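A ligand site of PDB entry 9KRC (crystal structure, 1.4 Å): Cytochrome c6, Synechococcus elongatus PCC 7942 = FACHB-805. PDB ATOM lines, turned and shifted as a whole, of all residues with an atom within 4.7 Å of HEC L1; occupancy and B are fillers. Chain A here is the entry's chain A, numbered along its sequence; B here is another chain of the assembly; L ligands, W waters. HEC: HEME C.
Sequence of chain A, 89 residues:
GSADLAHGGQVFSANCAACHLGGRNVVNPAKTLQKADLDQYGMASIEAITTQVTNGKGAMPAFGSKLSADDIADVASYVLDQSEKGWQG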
ATOM      1  N   ASN A  15      13.966 -10.526 -11.073  1.00  0.00           N
ATOM      2  CA  ASN A  15      12.588 -10.540 -10.631  1.00  0.00           C
ATOM      3  C   ASN A  15      12.302  -9.685  -9.419  1.00  0.00           C
ATOM      4  O   ASN A  15      11.142  -9.349  -9.191  1.00  0.00           O
ATOM      5  CB  ASN A  15      12.162 -11.974 -10.291  1.00  0.00           C
ATOM      6  CG  ASN A  15      12.154 -12.865 -11.508  1.00  0.00           C
ATOM      7  OD1 ASN A  15      11.227 -12.837 -12.301  1.00  0.00           O
ATOM      8  ND2 ASN A  15      13.225 -13.636 -11.680  1.00  0.00           N
ATOM      9  N   CYS A  16      13.310  -9.353  -8.632  1.00  0.00           N
ATOM     10  CA  CYS A  16      13.079  -8.722  -7.339  1.00  0.00           C
ATOM     11  C   CYS A  16      13.768  -7.383  -7.191  1.00  0.00           C
ATOM     12  O   CYS A  16      13.300  -6.538  -6.425  1.00  0.00           O
ATOM     13  CB  CYS A  16      13.566  -9.626  -6.199  1.00  0.00           C
ATOM     14  SG  CYS A  16      13.180 -11.366  -6.417  1.00  0.00           S
ATOM     15  N   CYS A  19      12.294  -3.740  -7.028  1.00  0.00           N
ATOM     16  CA  CYS A  19      11.707  -3.226  -5.805  1.00  0.00           C
ATOM     17  C   CYS A  19      12.565  -3.413  -4.586  1.00  0.00           C
ATOM     18  O   CYS A  19      12.385  -2.687  -3.613  1.00  0.00           O
ATOM     19  CB  CYS A  19      10.353  -3.894  -5.523  1.00  0.00           C
ATOM     20  SG  CYS A  19       9.180  -3.560  -6.838  1.00  0.00           S
ATOM     21  N   HIS A  20      13.500  -4.354  -4.602  1.00  0.00           N
ATOM     22  CA  HIS A  20      14.237  -4.755  -3.421  1.00  0.00           C
ATOM     23  C   HIS A  20      15.742  -4.628  -3.608  1.00  0.00           C
ATOM     24  O   HIS A  20      16.495  -5.306  -2.924  1.00  0.00           O
ATOM     25  CB  HIS A  20      13.903  -6.185  -2.986  1.00  0.00           C
ATOM     26  CG  HIS A  20      12.497  -6.394  -2.532  1.00  0.00           C
ATOM     27  ND1 HIS A  20      11.954  -5.764  -1.419  1.00  0.00           N
ATOM     28  CD2 HIS A  20      11.526  -7.237  -2.988  1.00  0.00           C
ATOM     29  CE1 HIS A  20      10.720  -6.205  -1.235  1.00  0.00           C
ATOM     30  NE2 HIS A  20      10.446  -7.102  -2.168  1.00  0.00           N
ATOM     31  N   ASN A  25      13.054  -1.790   0.134  1.00  0.00           N
ATOM     32  CA  ASN A  25      11.734  -1.999  -0.469  1.00  0.00           C
ATOM     33  C   ASN A  25      11.256  -0.627  -0.902  1.00  0.00           C
ATOM     34  O   ASN A  25      10.806   0.166  -0.066  1.00  0.00           O
ATOM     35  CB  ASN A  25      10.770  -2.634   0.527  1.00  0.00           C
ATOM     36  CG  ASN A  25       9.414  -2.931  -0.090  1.00  0.00           C
ATOM     37  OD1 ASN A  25       9.000  -2.300  -1.064  1.00  0.00           O
ATOM     38  ND2 ASN A  25       8.731  -3.914   0.459  1.00  0.00           N
ATOM     39  N   VAL A  27       8.739   0.325  -2.465  1.00  0.00           N
ATOM     40  CA  VAL A  27       7.301   0.561  -2.356  1.00  0.00           C
ATOM     41  C   VAL A  27       6.908   0.774  -0.904  1.00  0.00           C
ATOM     42  O   VAL A  27       6.123   1.676  -0.588  1.00  0.00           O
ATOM     43  CB  VAL A  27       6.545  -0.629  -2.976  1.00  0.00           C
ATOM     44  CG1 VAL A  27       5.045  -0.441  -2.829  1.00  0.00           C
ATOM     45  CG2 VAL A  27       6.926  -0.774  -4.443  1.00  0.00           C
ATOM     46  N   ASN A  28       7.468  -0.027  -0.001  1.00  0.00           N
ATOM     47  CA  ASN A  28       7.118   0.048   1.410  1.00  0.00           C
ATOM     48  C   ASN A  28       8.392  -0.077   2.217  1.00  0.00           C
ATOM     49  O   ASN A  28       8.836  -1.182   2.529  1.00  0.00           O
ATOM     50  CB  ASN A  28       6.129  -1.044   1.804  1.00  0.00           C
ATOM     51  CG  ASN A  28       5.631  -0.881   3.230  1.00  0.00           C
ATOM     52  OD1 ASN A  28       6.241  -0.171   4.029  1.00  0.00           O
ATOM     53  ND2 ASN A  28       4.521  -1.545   3.548  1.00  0.00           N
ATOM     54  N   LYS A  31       8.966  -2.559   5.121  1.00  0.00           N
ATOM     55  CA  LYS A  31       8.986  -3.997   4.899  1.00  0.00           C
ATOM     56  C   LYS A  31      10.143  -4.368   3.992  1.00  0.00           C
ATOM     57  O   LYS A  31       9.951  -4.894   2.888  1.00  0.00           O
ATOM     58  CB  LYS A  31       7.645  -4.456   4.342  1.00  0.00           C
ATOM     59  CG  LYS A  31       6.522  -4.349   5.399  1.00  0.00           C
ATOM     60  CD  LYS A  31       5.191  -4.871   4.899  1.00  0.00           C
ATOM     61  CE  LYS A  31       4.117  -4.694   5.949  1.00  0.00           C
ATOM     62  NZ  LYS A  31       2.769  -5.118   5.453  1.00  0.00           N
ATOM     63  N   THR A  32      11.362  -4.083   4.442  1.00  0.00           N
ATOM     64  CA  THR A  32      12.527  -4.374   3.633  1.00  0.00           C
ATOM     65  C   THR A  32      12.904  -5.844   3.782  1.00  0.00           C
ATOM     66  O   THR A  32      12.284  -6.605   4.516  1.00  0.00           O
ATOM     67  CB  THR A  32      13.719  -3.532   4.082  1.00  0.00           C
ATOM     68  OG1 THR A  32      14.193  -4.035   5.336  1.00  0.00           O
ATOM     69  CG2 THR A  32      13.358  -2.051   4.203  1.00  0.00           C
ATOM     70  N   LEU A  33      13.976  -6.232   3.108  1.00  0.00           N
ATOM     71  CA  LEU A  33      14.540  -7.555   3.276  1.00  0.00           C
ATOM     72  C   LEU A  33      15.664  -7.565   4.301  1.00  0.00           C
ATOM     73  O   LEU A  33      16.405  -8.543   4.375  1.00  0.00           O
ATOM     74  CB  LEU A  33      15.045  -8.115   1.948  1.00  0.00           C
ATOM     75  CG  LEU A  33      14.063  -7.956   0.785  1.00  0.00           C
ATOM     76  CD1 LEU A  33      14.573  -8.684  -0.426  1.00  0.00           C
ATOM     77  CD2 LEU A  33      12.685  -8.486   1.173  1.00  0.00           C
ATOM     78  N   ASP A  37      13.580  -6.534   9.776  1.00  0.00           N
ATOM     79  CA  ASP A  37      12.220  -6.561   9.246  1.00  0.00           C
ATOM     80  C   ASP A  37      11.759  -7.991   8.994  1.00  0.00           C
ATOM     81  O   ASP A  37      10.631  -8.346   9.337  1.00  0.00           O
ATOM     82  CB  ASP A  37      12.125  -5.729   7.963  1.00  0.00           C
ATOM     83  CG  ASP A  37      12.197  -4.240   8.218  1.00  0.00           C
ATOM     84  OD1 ASP A  37      12.078  -3.785   9.376  1.00  0.00           O
ATOM     85  OD2 ASP A  37      12.380  -3.495   7.222  1.00  0.00           O
ATOM     86  N   LEU A  38      12.599  -8.811   8.351  1.00  0.00           N
ATOM     87  CA  LEU A  38      12.203 -10.196   8.154  1.00  0.00           C
ATOM     88  C   LEU A  38      11.895 -10.878   9.480  1.00  0.00           C
ATOM     89  O   LEU A  38      10.918 -11.628   9.590  1.00  0.00           O
ATOM     90  CB  LEU A  38      13.279 -10.975   7.393  1.00  0.00           C
ATOM     91  CG  LEU A  38      13.586 -10.501   5.967  1.00  0.00           C
ATOM     92  CD1 LEU A  38      14.546 -11.500   5.324  1.00  0.00           C
ATOM     93  CD2 LEU A  38      12.334 -10.350   5.123  1.00  0.00           C
ATOM     94  N   TYR A  41       8.445  -9.567  10.973  1.00  0.00           N
ATOM     95  CA  TYR A  41       7.243  -9.971  10.265  1.00  0.00           C
ATOM     96  C   TYR A  41       7.171 -11.477  10.012  1.00  0.00           C
ATOM     97  O   TYR A  41       6.327 -11.924   9.228  1.00  0.00           O
ATOM     98  CB  TYR A  41       7.092  -9.170   8.969  1.00  0.00           C
ATOM     99  CG  TYR A  41       7.014  -7.688   9.213  1.00  0.00           C
ATOM    100  CD1 TYR A  41       5.956  -7.151   9.929  1.00  0.00           C
ATOM    101  CD2 TYR A  41       7.997  -6.825   8.743  1.00  0.00           C
ATOM    102  CE1 TYR A  41       5.870  -5.787  10.156  1.00  0.00           C
ATOM    103  CE2 TYR A  41       7.927  -5.472   8.971  1.00  0.00           C
ATOM    104  CZ  TYR A  41       6.862  -4.948   9.674  1.00  0.00           C
ATOM    105  OH  TYR A  41       6.788  -3.583   9.908  1.00  0.00           O
ATOM    106  N   MET A  43       9.209 -13.421   8.420  1.00  0.00           N
ATOM    107  CA  MET A  43       9.563 -13.679   7.035  1.00  0.00           C
ATOM    108  C   MET A  43      10.987 -14.170   6.881  1.00  0.00           C
ATOM    109  O   MET A  43      11.500 -14.232   5.758  1.00  0.00           O
ATOM    110  CB  MET A  43       9.315 -12.424   6.201  1.00  0.00           C
ATOM    111  CG  MET A  43       7.852 -12.089   6.029  1.00  0.00           C
ATOM    112  SD  MET A  43       6.930 -13.334   5.104  1.00  0.00           S
ATOM    113  CE  MET A  43       7.811 -13.336   3.553  1.00  0.00           C
ATOM    114  N   ILE A  49       9.414 -16.972   2.774  1.00  0.00           N
ATOM    115  CA  ILE A  49       9.783 -16.236   1.572  1.00  0.00           C
ATOM    116  C   ILE A  49       9.236 -16.921   0.331  1.00  0.00           C
ATOM    117  O   ILE A  49       8.660 -16.263  -0.544  1.00  0.00           O
ATOM    118  CB  ILE A  49      11.312 -16.039   1.500  1.00  0.00           C
ATOM    119  CG1 ILE A  49      11.811 -15.221   2.684  1.00  0.00           C
ATOM    120  CG2 ILE A  49      11.669 -15.374   0.177  1.00  0.00           C
ATOM    121  CD1 ILE A  49      13.315 -15.361   2.944  1.00  0.00           C
ATOM    122  N   GLN A  52       5.473 -16.203   0.005  1.00  0.00           N
ATOM    123  CA  GLN A  52       5.117 -14.847  -0.409  1.00  0.00           C
ATOM    124  C   GLN A  52       5.552 -14.575  -1.831  1.00  0.00           C
ATOM    125  O   GLN A  52       4.853 -13.881  -2.579  1.00  0.00           O
ATOM    126  CB  GLN A  52       5.679 -13.829   0.571  1.00  0.00           C
ATOM    127  CG  GLN A  52       5.230 -12.419   0.234  1.00  0.00           C
ATOM    128  CD  GLN A  52       5.186 -11.519   1.428  1.00  0.00           C
ATOM    129  OE1 GLN A  52       4.734 -11.921   2.486  1.00  0.00           O
ATOM    130  NE2 GLN A  52       5.664 -10.299   1.268  1.00  0.00           N
ATOM    131  N   VAL A  53       6.703 -15.128  -2.251  1.00  0.00           N
ATOM    132  CA  VAL A  53       7.084 -14.999  -3.653  1.00  0.00           C
ATOM    133  C   VAL A  53       6.065 -15.695  -4.545  1.00  0.00           C
ATOM    134  O   VAL A  53       5.679 -15.176  -5.592  1.00  0.00           O
ATOM    135  CB  VAL A  53       8.494 -15.553  -3.858  1.00  0.00           C
ATOM    136  CG1 VAL A  53       8.810 -15.671  -5.343  1.00  0.00           C
ATOM    137  CG2 VAL A  53       9.499 -14.647  -3.180  1.00  0.00           C
ATOM    138  N   LYS A  57       1.763 -10.513  -2.260  1.00  0.00           N
ATOM    139  CA  LYS A  57       1.103  -9.985  -1.069  1.00  0.00           C
ATOM    140  C   LYS A  57       0.979  -8.487  -1.227  1.00  0.00           C
ATOM    141  O   LYS A  57       1.968  -7.807  -1.458  1.00  0.00           O
ATOM    142  CB  LYS A  57       1.890 -10.300   0.211  1.00  0.00           C
ATOM    143  CG  LYS A  57       1.147  -9.797   1.445  1.00  0.00           C
ATOM    144  CD  LYS A  57       1.824 -10.197   2.737  1.00  0.00           C
ATOM    145  CE  LYS A  57       1.094  -9.577   3.924  1.00  0.00           C
ATOM    146  NZ  LYS A  57       1.701  -9.937   5.217  1.00  0.00           N
ATOM    147  N   GLY A  58      -0.240  -7.969  -1.098  1.00  0.00           N
ATOM    148  CA  GLY A  58      -0.409  -6.532  -1.229  1.00  0.00           C
ATOM    149  C   GLY A  58       0.084  -6.061  -2.578  1.00  0.00           C
ATOM    150  O   GLY A  58      -0.265  -6.610  -3.628  1.00  0.00           O
ATOM    151  N   ALA A  59       0.929  -5.025  -2.558  1.00  0.00           N
ATOM    152  CA  ALA A  59       1.480  -4.489  -3.791  1.00  0.00           C
ATOM    153  C   ALA A  59       2.588  -5.356  -4.378  1.00  0.00           C
ATOM    154  O   ALA A  59       3.046  -5.075  -5.488  1.00  0.00           O
ATOM    155  CB  ALA A  59       2.018  -3.089  -3.555  1.00  0.00           C
ATOM    156  N   MET A  60       3.040  -6.392  -3.682  1.00  0.00           N
ATOM    157  CA  MET A  60       4.061  -7.273  -4.235  1.00  0.00           C
ATOM    158  C   MET A  60       3.416  -8.281  -5.176  1.00  0.00           C
ATOM    159  O   MET A  60       2.516  -9.016  -4.759  1.00  0.00           O
ATOM    160  CB  MET A  60       4.794  -8.006  -3.134  1.00  0.00           C
ATOM    161  CG  MET A  60       5.759  -9.022  -3.704  1.00  0.00           C
ATOM    162  SD  MET A  60       6.879  -9.617  -2.448  1.00  0.00           S
ATOM    163  CE  MET A  60       7.286 -11.235  -3.116  1.00  0.00           C
ATOM    164  N   PRO A  61       3.872  -8.373  -6.418  1.00  0.00           N
ATOM    165  CA  PRO A  61       3.316  -9.374  -7.342  1.00  0.00           C
ATOM    166  C   PRO A  61       3.610 -10.797  -6.903  1.00  0.00           C
ATOM    167  O   PRO A  61       4.519 -11.081  -6.120  1.00  0.00           O
ATOM    168  CB  PRO A  61       4.010  -9.069  -8.675  1.00  0.00           C
ATOM    169  CG  PRO A  61       5.055  -8.076  -8.395  1.00  0.00           C
ATOM    170  CD  PRO A  61       4.848  -7.492  -7.054  1.00  0.00           C
ATOM    171  N   PHE A  63       4.722 -14.627  -8.146  1.00  0.00           N
ATOM    172  CA  PHE A  63       5.656 -15.233  -9.086  1.00  0.00           C
ATOM    173  C   PHE A  63       5.423 -16.716  -9.282  1.00  0.00           C
ATOM    174  O   PHE A  63       6.187 -17.359 -10.010  1.00  0.00           O
ATOM    175  CB  PHE A  63       7.099 -15.010  -8.615  1.00  0.00           C
ATOM    176  CG  PHE A  63       7.497 -13.563  -8.602  1.00  0.00           C
ATOM    177  CD1 PHE A  63       7.166 -12.756  -7.529  1.00  0.00           C
ATOM    178  CD2 PHE A  63       8.165 -12.995  -9.692  1.00  0.00           C
ATOM    179  CE1 PHE A  63       7.516 -11.415  -7.521  1.00  0.00           C
ATOM    180  CE2 PHE A  63       8.511 -11.660  -9.690  1.00  0.00           C
ATOM    181  CZ  PHE A  63       8.189 -10.858  -8.602  1.00  0.00           C
ATOM    182  N   LEU A  67       7.961 -18.570 -12.262  1.00  0.00           N
ATOM    183  CA  LEU A  67       9.229 -19.148 -11.857  1.00  0.00           C
ATOM    184  C   LEU A  67       9.035 -20.595 -11.473  1.00  0.00           C
ATOM    185  O   LEU A  67       7.983 -20.989 -10.954  1.00  0.00           O
ATOM    186  CB  LEU A  67       9.772 -18.385 -10.646  1.00  0.00           C
ATOM    187  CG  LEU A  67      10.126 -16.919 -10.899  1.00  0.00           C
ATOM    188  CD1 LEU A  67      10.598 -16.282  -9.613  1.00  0.00           C
ATOM    189  CD2 LEU A  67      11.180 -16.798 -11.988  1.00  0.00           C
ATOM    190  N   VAL A  75      15.822 -18.234  -4.875  1.00  0.00           N
ATOM    191  CA  VAL A  75      15.769 -16.822  -4.517  1.00  0.00           C
ATOM    192  C   VAL A  75      15.506 -16.646  -3.028  1.00  0.00           C
ATOM    193  O   VAL A  75      16.038 -15.722  -2.395  1.00  0.00           O
ATOM    194  CB  VAL A  75      14.809 -16.016  -5.419  1.00  0.00           C
ATOM    195  CG1 VAL A  75      13.345 -16.217  -5.046  1.00  0.00           C
ATOM    196  CG2 VAL A  75      15.169 -14.547  -5.359  1.00  0.00           C
ATOM    197  N   VAL A  79      17.847 -14.545  -0.554  1.00  0.00           N
ATOM    198  CA  VAL A  79      17.347 -13.470   0.309  1.00  0.00           C
ATOM    199  C   VAL A  79      17.732 -13.721   1.762  1.00  0.00           C
ATOM    200  O   VAL A  79      18.209 -12.830   2.460  1.00  0.00           O
ATOM    201  CB  VAL A  79      15.820 -13.314   0.138  1.00  0.00           C
ATOM    202  CG1 VAL A  79      15.250 -12.456   1.270  1.00  0.00           C
ATOM    203  CG2 VAL A  79      15.488 -12.730  -1.234  1.00  0.00           C
ATOM    204  N   VAL B  27       8.173   2.610  -9.032  1.00  0.00           N
ATOM    205  CA  VAL B  27       8.970   1.450  -9.422  1.00  0.00           C
ATOM    206  C   VAL B  27       9.635   1.695 -10.770  1.00  0.00           C
ATOM    207  O   VAL B  27      10.752   1.205 -11.033  1.00  0.00           O
ATOM    208  CB  VAL B  27       8.064   0.207  -9.429  1.00  0.00           C
ATOM    209  CG1 VAL B  27       8.843  -1.026  -9.904  1.00  0.00           C
ATOM    210  CG2 VAL B  27       7.484  -0.036  -8.057  1.00  0.00           C
ATOM    211  N   ALA B  59       6.694  -5.811 -12.965  1.00  0.00           N
ATOM    212  CA  ALA B  59       6.649  -5.593 -11.523  1.00  0.00           C
ATOM    213  C   ALA B  59       5.289  -5.105 -11.054  1.00  0.00           C
ATOM    214  O   ALA B  59       5.075  -5.021  -9.839  1.00  0.00           O
ATOM    215  CB  ALA B  59       7.739  -4.603 -11.100  1.00  0.00           C
HETATM  216 FE   HEC L   1       8.811  -8.243  -2.365  1.00  0.00          FE
HETATM  217  CHA HEC L   1       7.613  -7.810   0.789  1.00  0.00           C
HETATM  218  CHB HEC L   1      10.684 -10.906  -1.294  1.00  0.00           C
HETATM  219  CHC HEC L   1       9.745  -8.882  -5.542  1.00  0.00           C
HETATM  220  CHD HEC L   1       7.368  -5.325  -3.379  1.00  0.00           C
HETATM  221  NA  HEC L   1       9.115  -9.159  -0.605  1.00  0.00           N
HETATM  222  C1A HEC L   1       8.562  -8.793   0.592  1.00  0.00           C
HETATM  223  C2A HEC L   1       9.101  -9.637   1.641  1.00  0.00           C
HETATM  224  C3A HEC L   1       9.936 -10.492   1.051  1.00  0.00           C
HETATM  225  C4A HEC L   1       9.950 -10.225  -0.363  1.00  0.00           C
HETATM  226  CMA HEC L   1      10.785 -11.595   1.717  1.00  0.00           C
HETATM  227  CAA HEC L   1       8.780  -9.505   3.147  1.00  0.00           C
HETATM  228  CBA HEC L   1       9.569  -8.286   3.658  1.00  0.00           C
HETATM  229  CGA HEC L   1       9.298  -7.985   5.119  1.00  0.00           C
HETATM  230  O1A HEC L   1      10.019  -7.127   5.722  1.00  0.00           O
HETATM  231  O2A HEC L   1       8.363  -8.588   5.699  1.00  0.00           O
HETATM  232  NB  HEC L   1       9.942  -9.643  -3.232  1.00  0.00           N
HETATM  233  C1B HEC L   1      10.651 -10.662  -2.643  1.00  0.00           C
HETATM  234  C2B HEC L   1      11.204 -11.509  -3.669  1.00  0.00           C
HETATM  235  C3B HEC L   1      10.989 -10.922  -4.838  1.00  0.00           C
HETATM  236  C4B HEC L   1      10.152  -9.770  -4.585  1.00  0.00           C
HETATM  237  CMB HEC L   1      12.151 -12.684  -3.355  1.00  0.00           C
HETATM  238  CAB HEC L   1      11.422 -11.368  -6.251  1.00  0.00           C
HETATM  239  CBB HEC L   1      10.899 -12.795  -6.576  1.00  0.00           C
HETATM  240  NC  HEC L   1       8.603  -7.290  -4.098  1.00  0.00           N
HETATM  241  C1C HEC L   1       9.100  -7.704  -5.306  1.00  0.00           C
HETATM  242  C2C HEC L   1       8.675  -6.801  -6.344  1.00  0.00           C
HETATM  243  C3C HEC L   1       8.085  -5.771  -5.750  1.00  0.00           C
HETATM  244  C4C HEC L   1       7.993  -6.060  -4.329  1.00  0.00           C
HETATM  245  CMC HEC L   1       9.109  -6.854  -7.825  1.00  0.00           C
HETATM  246  CAC HEC L   1       7.667  -4.435  -6.412  1.00  0.00           C
HETATM  247  CBC HEC L   1       6.546  -4.503  -7.407  1.00  0.00           C
HETATM  248  ND  HEC L   1       7.707  -6.817  -1.465  1.00  0.00           N
HETATM  249  C1D HEC L   1       7.098  -5.752  -2.113  1.00  0.00           C
HETATM  250  C2D HEC L   1       6.130  -5.154  -1.252  1.00  0.00           C
HETATM  251  C3D HEC L   1       6.199  -5.915   0.038  1.00  0.00           C
HETATM  252  C4D HEC L   1       7.198  -6.934  -0.168  1.00  0.00           C
HETATM  253  CMD HEC L   1       5.204  -3.969  -1.573  1.00  0.00           C
HETATM  254  CAD HEC L   1       5.299  -5.692   1.260  1.00  0.00           C
HETATM  255  CBD HEC L   1       4.023  -6.503   0.997  1.00  0.00           C
HETATM  256  CGD HEC L   1       3.053  -6.376   2.127  1.00  0.00           C
HETATM  257  O1D HEC L   1       3.303  -6.925   3.223  1.00  0.00           O
HETATM  258  O2D HEC L   1       2.015  -5.702   1.919  1.00  0.00           O
HETATM  259 FE   HEC L   2       0.769   0.187 -12.329  1.00  0.00          FE
HETATM  260  CHA HEC L   2       2.423   0.438 -15.269  1.00  0.00           C
HETATM  261  CHB HEC L   2      -2.058   1.427 -13.797  1.00  0.00           C
HETATM  262  CHC HEC L   2      -0.960  -0.336  -9.442  1.00  0.00           C
HETATM  263  CHD HEC L   2       3.675  -0.616 -10.684  1.00  0.00           C
HETATM  264  NA  HEC L   2       0.297   0.833 -14.181  1.00  0.00           N
HETATM  265  C1A HEC L   2       1.147   0.908 -15.258  1.00  0.00           C
HETATM  266  C2A HEC L   2       0.451   1.538 -16.354  1.00  0.00           C
HETATM  267  C3A HEC L   2      -0.788   1.789 -15.935  1.00  0.00           C
HETATM  268  C4A HEC L   2      -0.927   1.354 -14.572  1.00  0.00           C
HETATM  269  CMA HEC L   2      -1.897   2.447 -16.755  1.00  0.00           C
HETATM  270  CAA HEC L   2       1.089   1.844 -17.731  1.00  0.00           C
HETATM  271  CBA HEC L   2       1.899   3.133 -17.560  1.00  0.00           C
HETATM  272  CGA HEC L   2       2.736   3.468 -18.778  1.00  0.00           C
HETATM  273  O1A HEC L   2       3.313   4.583 -18.831  1.00  0.00           O
HETATM  274  O2A HEC L   2       2.825   2.634 -19.713  1.00  0.00           O
HETATM  275  NB  HEC L   2      -1.104   0.449 -11.746  1.00  0.00           N
HETATM  276  C1B HEC L   2      -2.157   0.950 -12.506  1.00  0.00           C
HETATM  277  C2B HEC L   2      -3.384   0.810 -11.769  1.00  0.00           C
HETATM  278  C3B HEC L   2      -3.073   0.385 -10.543  1.00  0.00           C
HETATM  279  C4B HEC L   2      -1.655   0.103 -10.533  1.00  0.00           C
HETATM  280  CMB HEC L   2      -4.706   1.416 -12.307  1.00  0.00           C
HETATM  281  CAB HEC L   2      -3.992   0.125  -9.336  1.00  0.00           C
HETATM  282  CBB HEC L   2      -5.117  -0.885  -9.672  1.00  0.00           C
HETATM  283  NC  HEC L   2       1.256  -0.379 -10.442  1.00  0.00           N
HETATM  284  C1C HEC L   2       0.386  -0.484  -9.371  1.00  0.00           C
HETATM  285  C2C HEC L   2       1.109  -1.000  -8.236  1.00  0.00           C
HETATM  286  C3C HEC L   2       2.409  -0.955  -8.541  1.00  0.00           C
HETATM  287  C4C HEC L   2       2.520  -0.617  -9.945  1.00  0.00           C
HETATM  288  CMC HEC L   2       0.527  -1.133  -6.818  1.00  0.00           C
HETATM  289  CAC HEC L   2       3.614  -1.193  -7.597  1.00  0.00           C
HETATM  290  CBC HEC L   2       3.725  -2.598  -7.037  1.00  0.00           C
HETATM  291  ND  HEC L   2       2.698  -0.022 -12.859  1.00  0.00           N
HETATM  292  C1D HEC L   2       3.724  -0.484 -12.047  1.00  0.00           C
HETATM  293  C2D HEC L   2       4.841  -0.827 -12.852  1.00  0.00           C
HETATM  294  C3D HEC L   2       4.471  -0.514 -14.268  1.00  0.00           C
HETATM  295  C4D HEC L   2       3.119  -0.019 -14.190  1.00  0.00           C
HETATM  296  CMD HEC L   2       6.203  -1.392 -12.438  1.00  0.00           C
HETATM  297  CAD HEC L   2       5.343  -0.761 -15.495  1.00  0.00           C
HETATM  298  CBD HEC L   2       5.110  -2.245 -15.813  1.00  0.00           C
HETATM  299  CGD HEC L   2       5.932  -2.644 -16.998  1.00  0.00           C
HETATM  300  O1D HEC L   2       5.561  -2.274 -18.135  1.00  0.00           O
HETATM  301  O2D HEC L   2       6.958  -3.354 -16.793  1.00  0.00           O
HETATM  302  O   HOH W   1       1.945  -2.951   3.555  1.00  0.00           O
HETATM  303  O   HOH W   2       5.683  -8.837   6.011  1.00  0.00           O
HETATM  304  O   HOH W   3       1.532  -4.013   0.002  1.00  0.00           O
HETATM  305  O   HOH W   4       5.429  -8.439   3.331  1.00  0.00           O
HETATM  306  O   HOH W   5      -0.290  -6.113   3.191  1.00  0.00           O
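Asn 15 touches HEC L1 (O to CMC, 3.5 Å). Asn 25 touches HEC L1. CG1 of Val 27 of chain A touches CMD of HEC L1 (3.7 Å). Leu 33 touches HEC L1 (CD2 to C3A, 3.4 Å). Asp 37 touches HEC L1. CD2 of Leu 38 touches CBA of HEC L1 (3.7 Å). Tyr 41 touches HEC L1. Met 43 touches HEC L1. Ile 49 touches HEC L1 (CG1 to CMA, 3.9 Å). Gln 52 touches HEC L1. Val 53 touches HEC L1. CB of Ala 59 of chain A touches CMD of HEC L1, 3.9 Å away. Pro 61 touches HEC L1 (CD to CBC, 3.5 Å). Phe 63 touches HEC L1 (CE1 to CBB, 3.8 Å). Val 79 touches HEC L1 (CG2 to CMB, 3.95 Å). O of Ala 59 of chain B touches CBC of HEC L1 (2.9 Å). Hydrophobic or aromatic side chains within 4 Å of HEC L1: His 20, Val 27 of chain A, Leu 33, Leu 38, Tyr 41, Met 43, Ile 49, Val 53, Ala 59 of chain A, Met 60, Pro 61, Phe 63, Val 79 and Ala 59 of chain B. 23 residues have an atom within 4 Å of HEC L1: Asn 15, Cys 16, Cys 19, His 20, Asn 25, Val 27 of chain A, Lys 31, Thr 32, Leu 33, Asp 37, Leu 38, Tyr 41, Met 43, Ile 49, Gln 52, Val 53, Lys 57, Ala 59 of chain A, Met 60, Pro 61, Phe 63, Val 79 and Ala 59 of chain B. Along chain A the residues within 4 Å of HEC L1 span positions 15 to 79.
The side-chain carboxylate (OD2) of Asp 37 sits at hydrogen-bond distance from the side-chain hydroxyl (OG1) of Thr 32, at 2.7 Å. The backbone NH (N) of Met 43 is in hydrogen-bond range of the backbone carbonyl oxygen (O) of Leu 38. SD of Met 43 lies close to OE1 of Gln 52. OD1 of Asn 25 lies within hydrogen-bond range of N of Val 27 of chain A, at 3.0 Å. The backbone carbonyl oxygen (O) of Lys 31 sits at hydrogen-bond distance from the side-chain amide nitrogen (ND2) of Asn 25, at 2.9 Å. The backbone NH of Asn 28 sits at hydrogen-bond distance from the side-chain amide oxygen of Asn 25 (2.9 Å). N of Phe 63 lies within hydrogen-bond range of O of Val 53.
O1A of HEC L1 lies close to O of Thr 32. SD of Met 60 is bound to FE of HEC L1 (2.4 Å). The side-chain amino group (NZ) of Lys 31 lies within salt-bridge range of an oxygen (O1D) of HEC L1 (2.9 Å). An oxygen (O1D) of HEC L1 is in salt-bridge range of the side-chain amino group (NZ) of Lys 57 (3.95 Å). CAB of HEC L1 is bonded to SG of Cys 16 (1.8 Å). FE of HEC L1 is bound by NE2 of His 20 (2.0 Å). A carbon (CAC) of HEC L1 is bonded to the side-chain sulfur (SG) of Cys 19.
Water W3 lies within hydrogen-bond range of an oxygen (O2D) of HEC L1 and the backbone NH (N) of Ala 59 of chain A. Water W4 bridges O1D of HEC L1 (2.6 Å) and NE2 of Gln 52 (2.8 Å). Water W1 lies within hydrogen-bond range of ND2 of Asn 28 (2.9 Å), NZ of Lys 31 (3.0 Å) and O2D of HEC L1 (3.2 Å).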
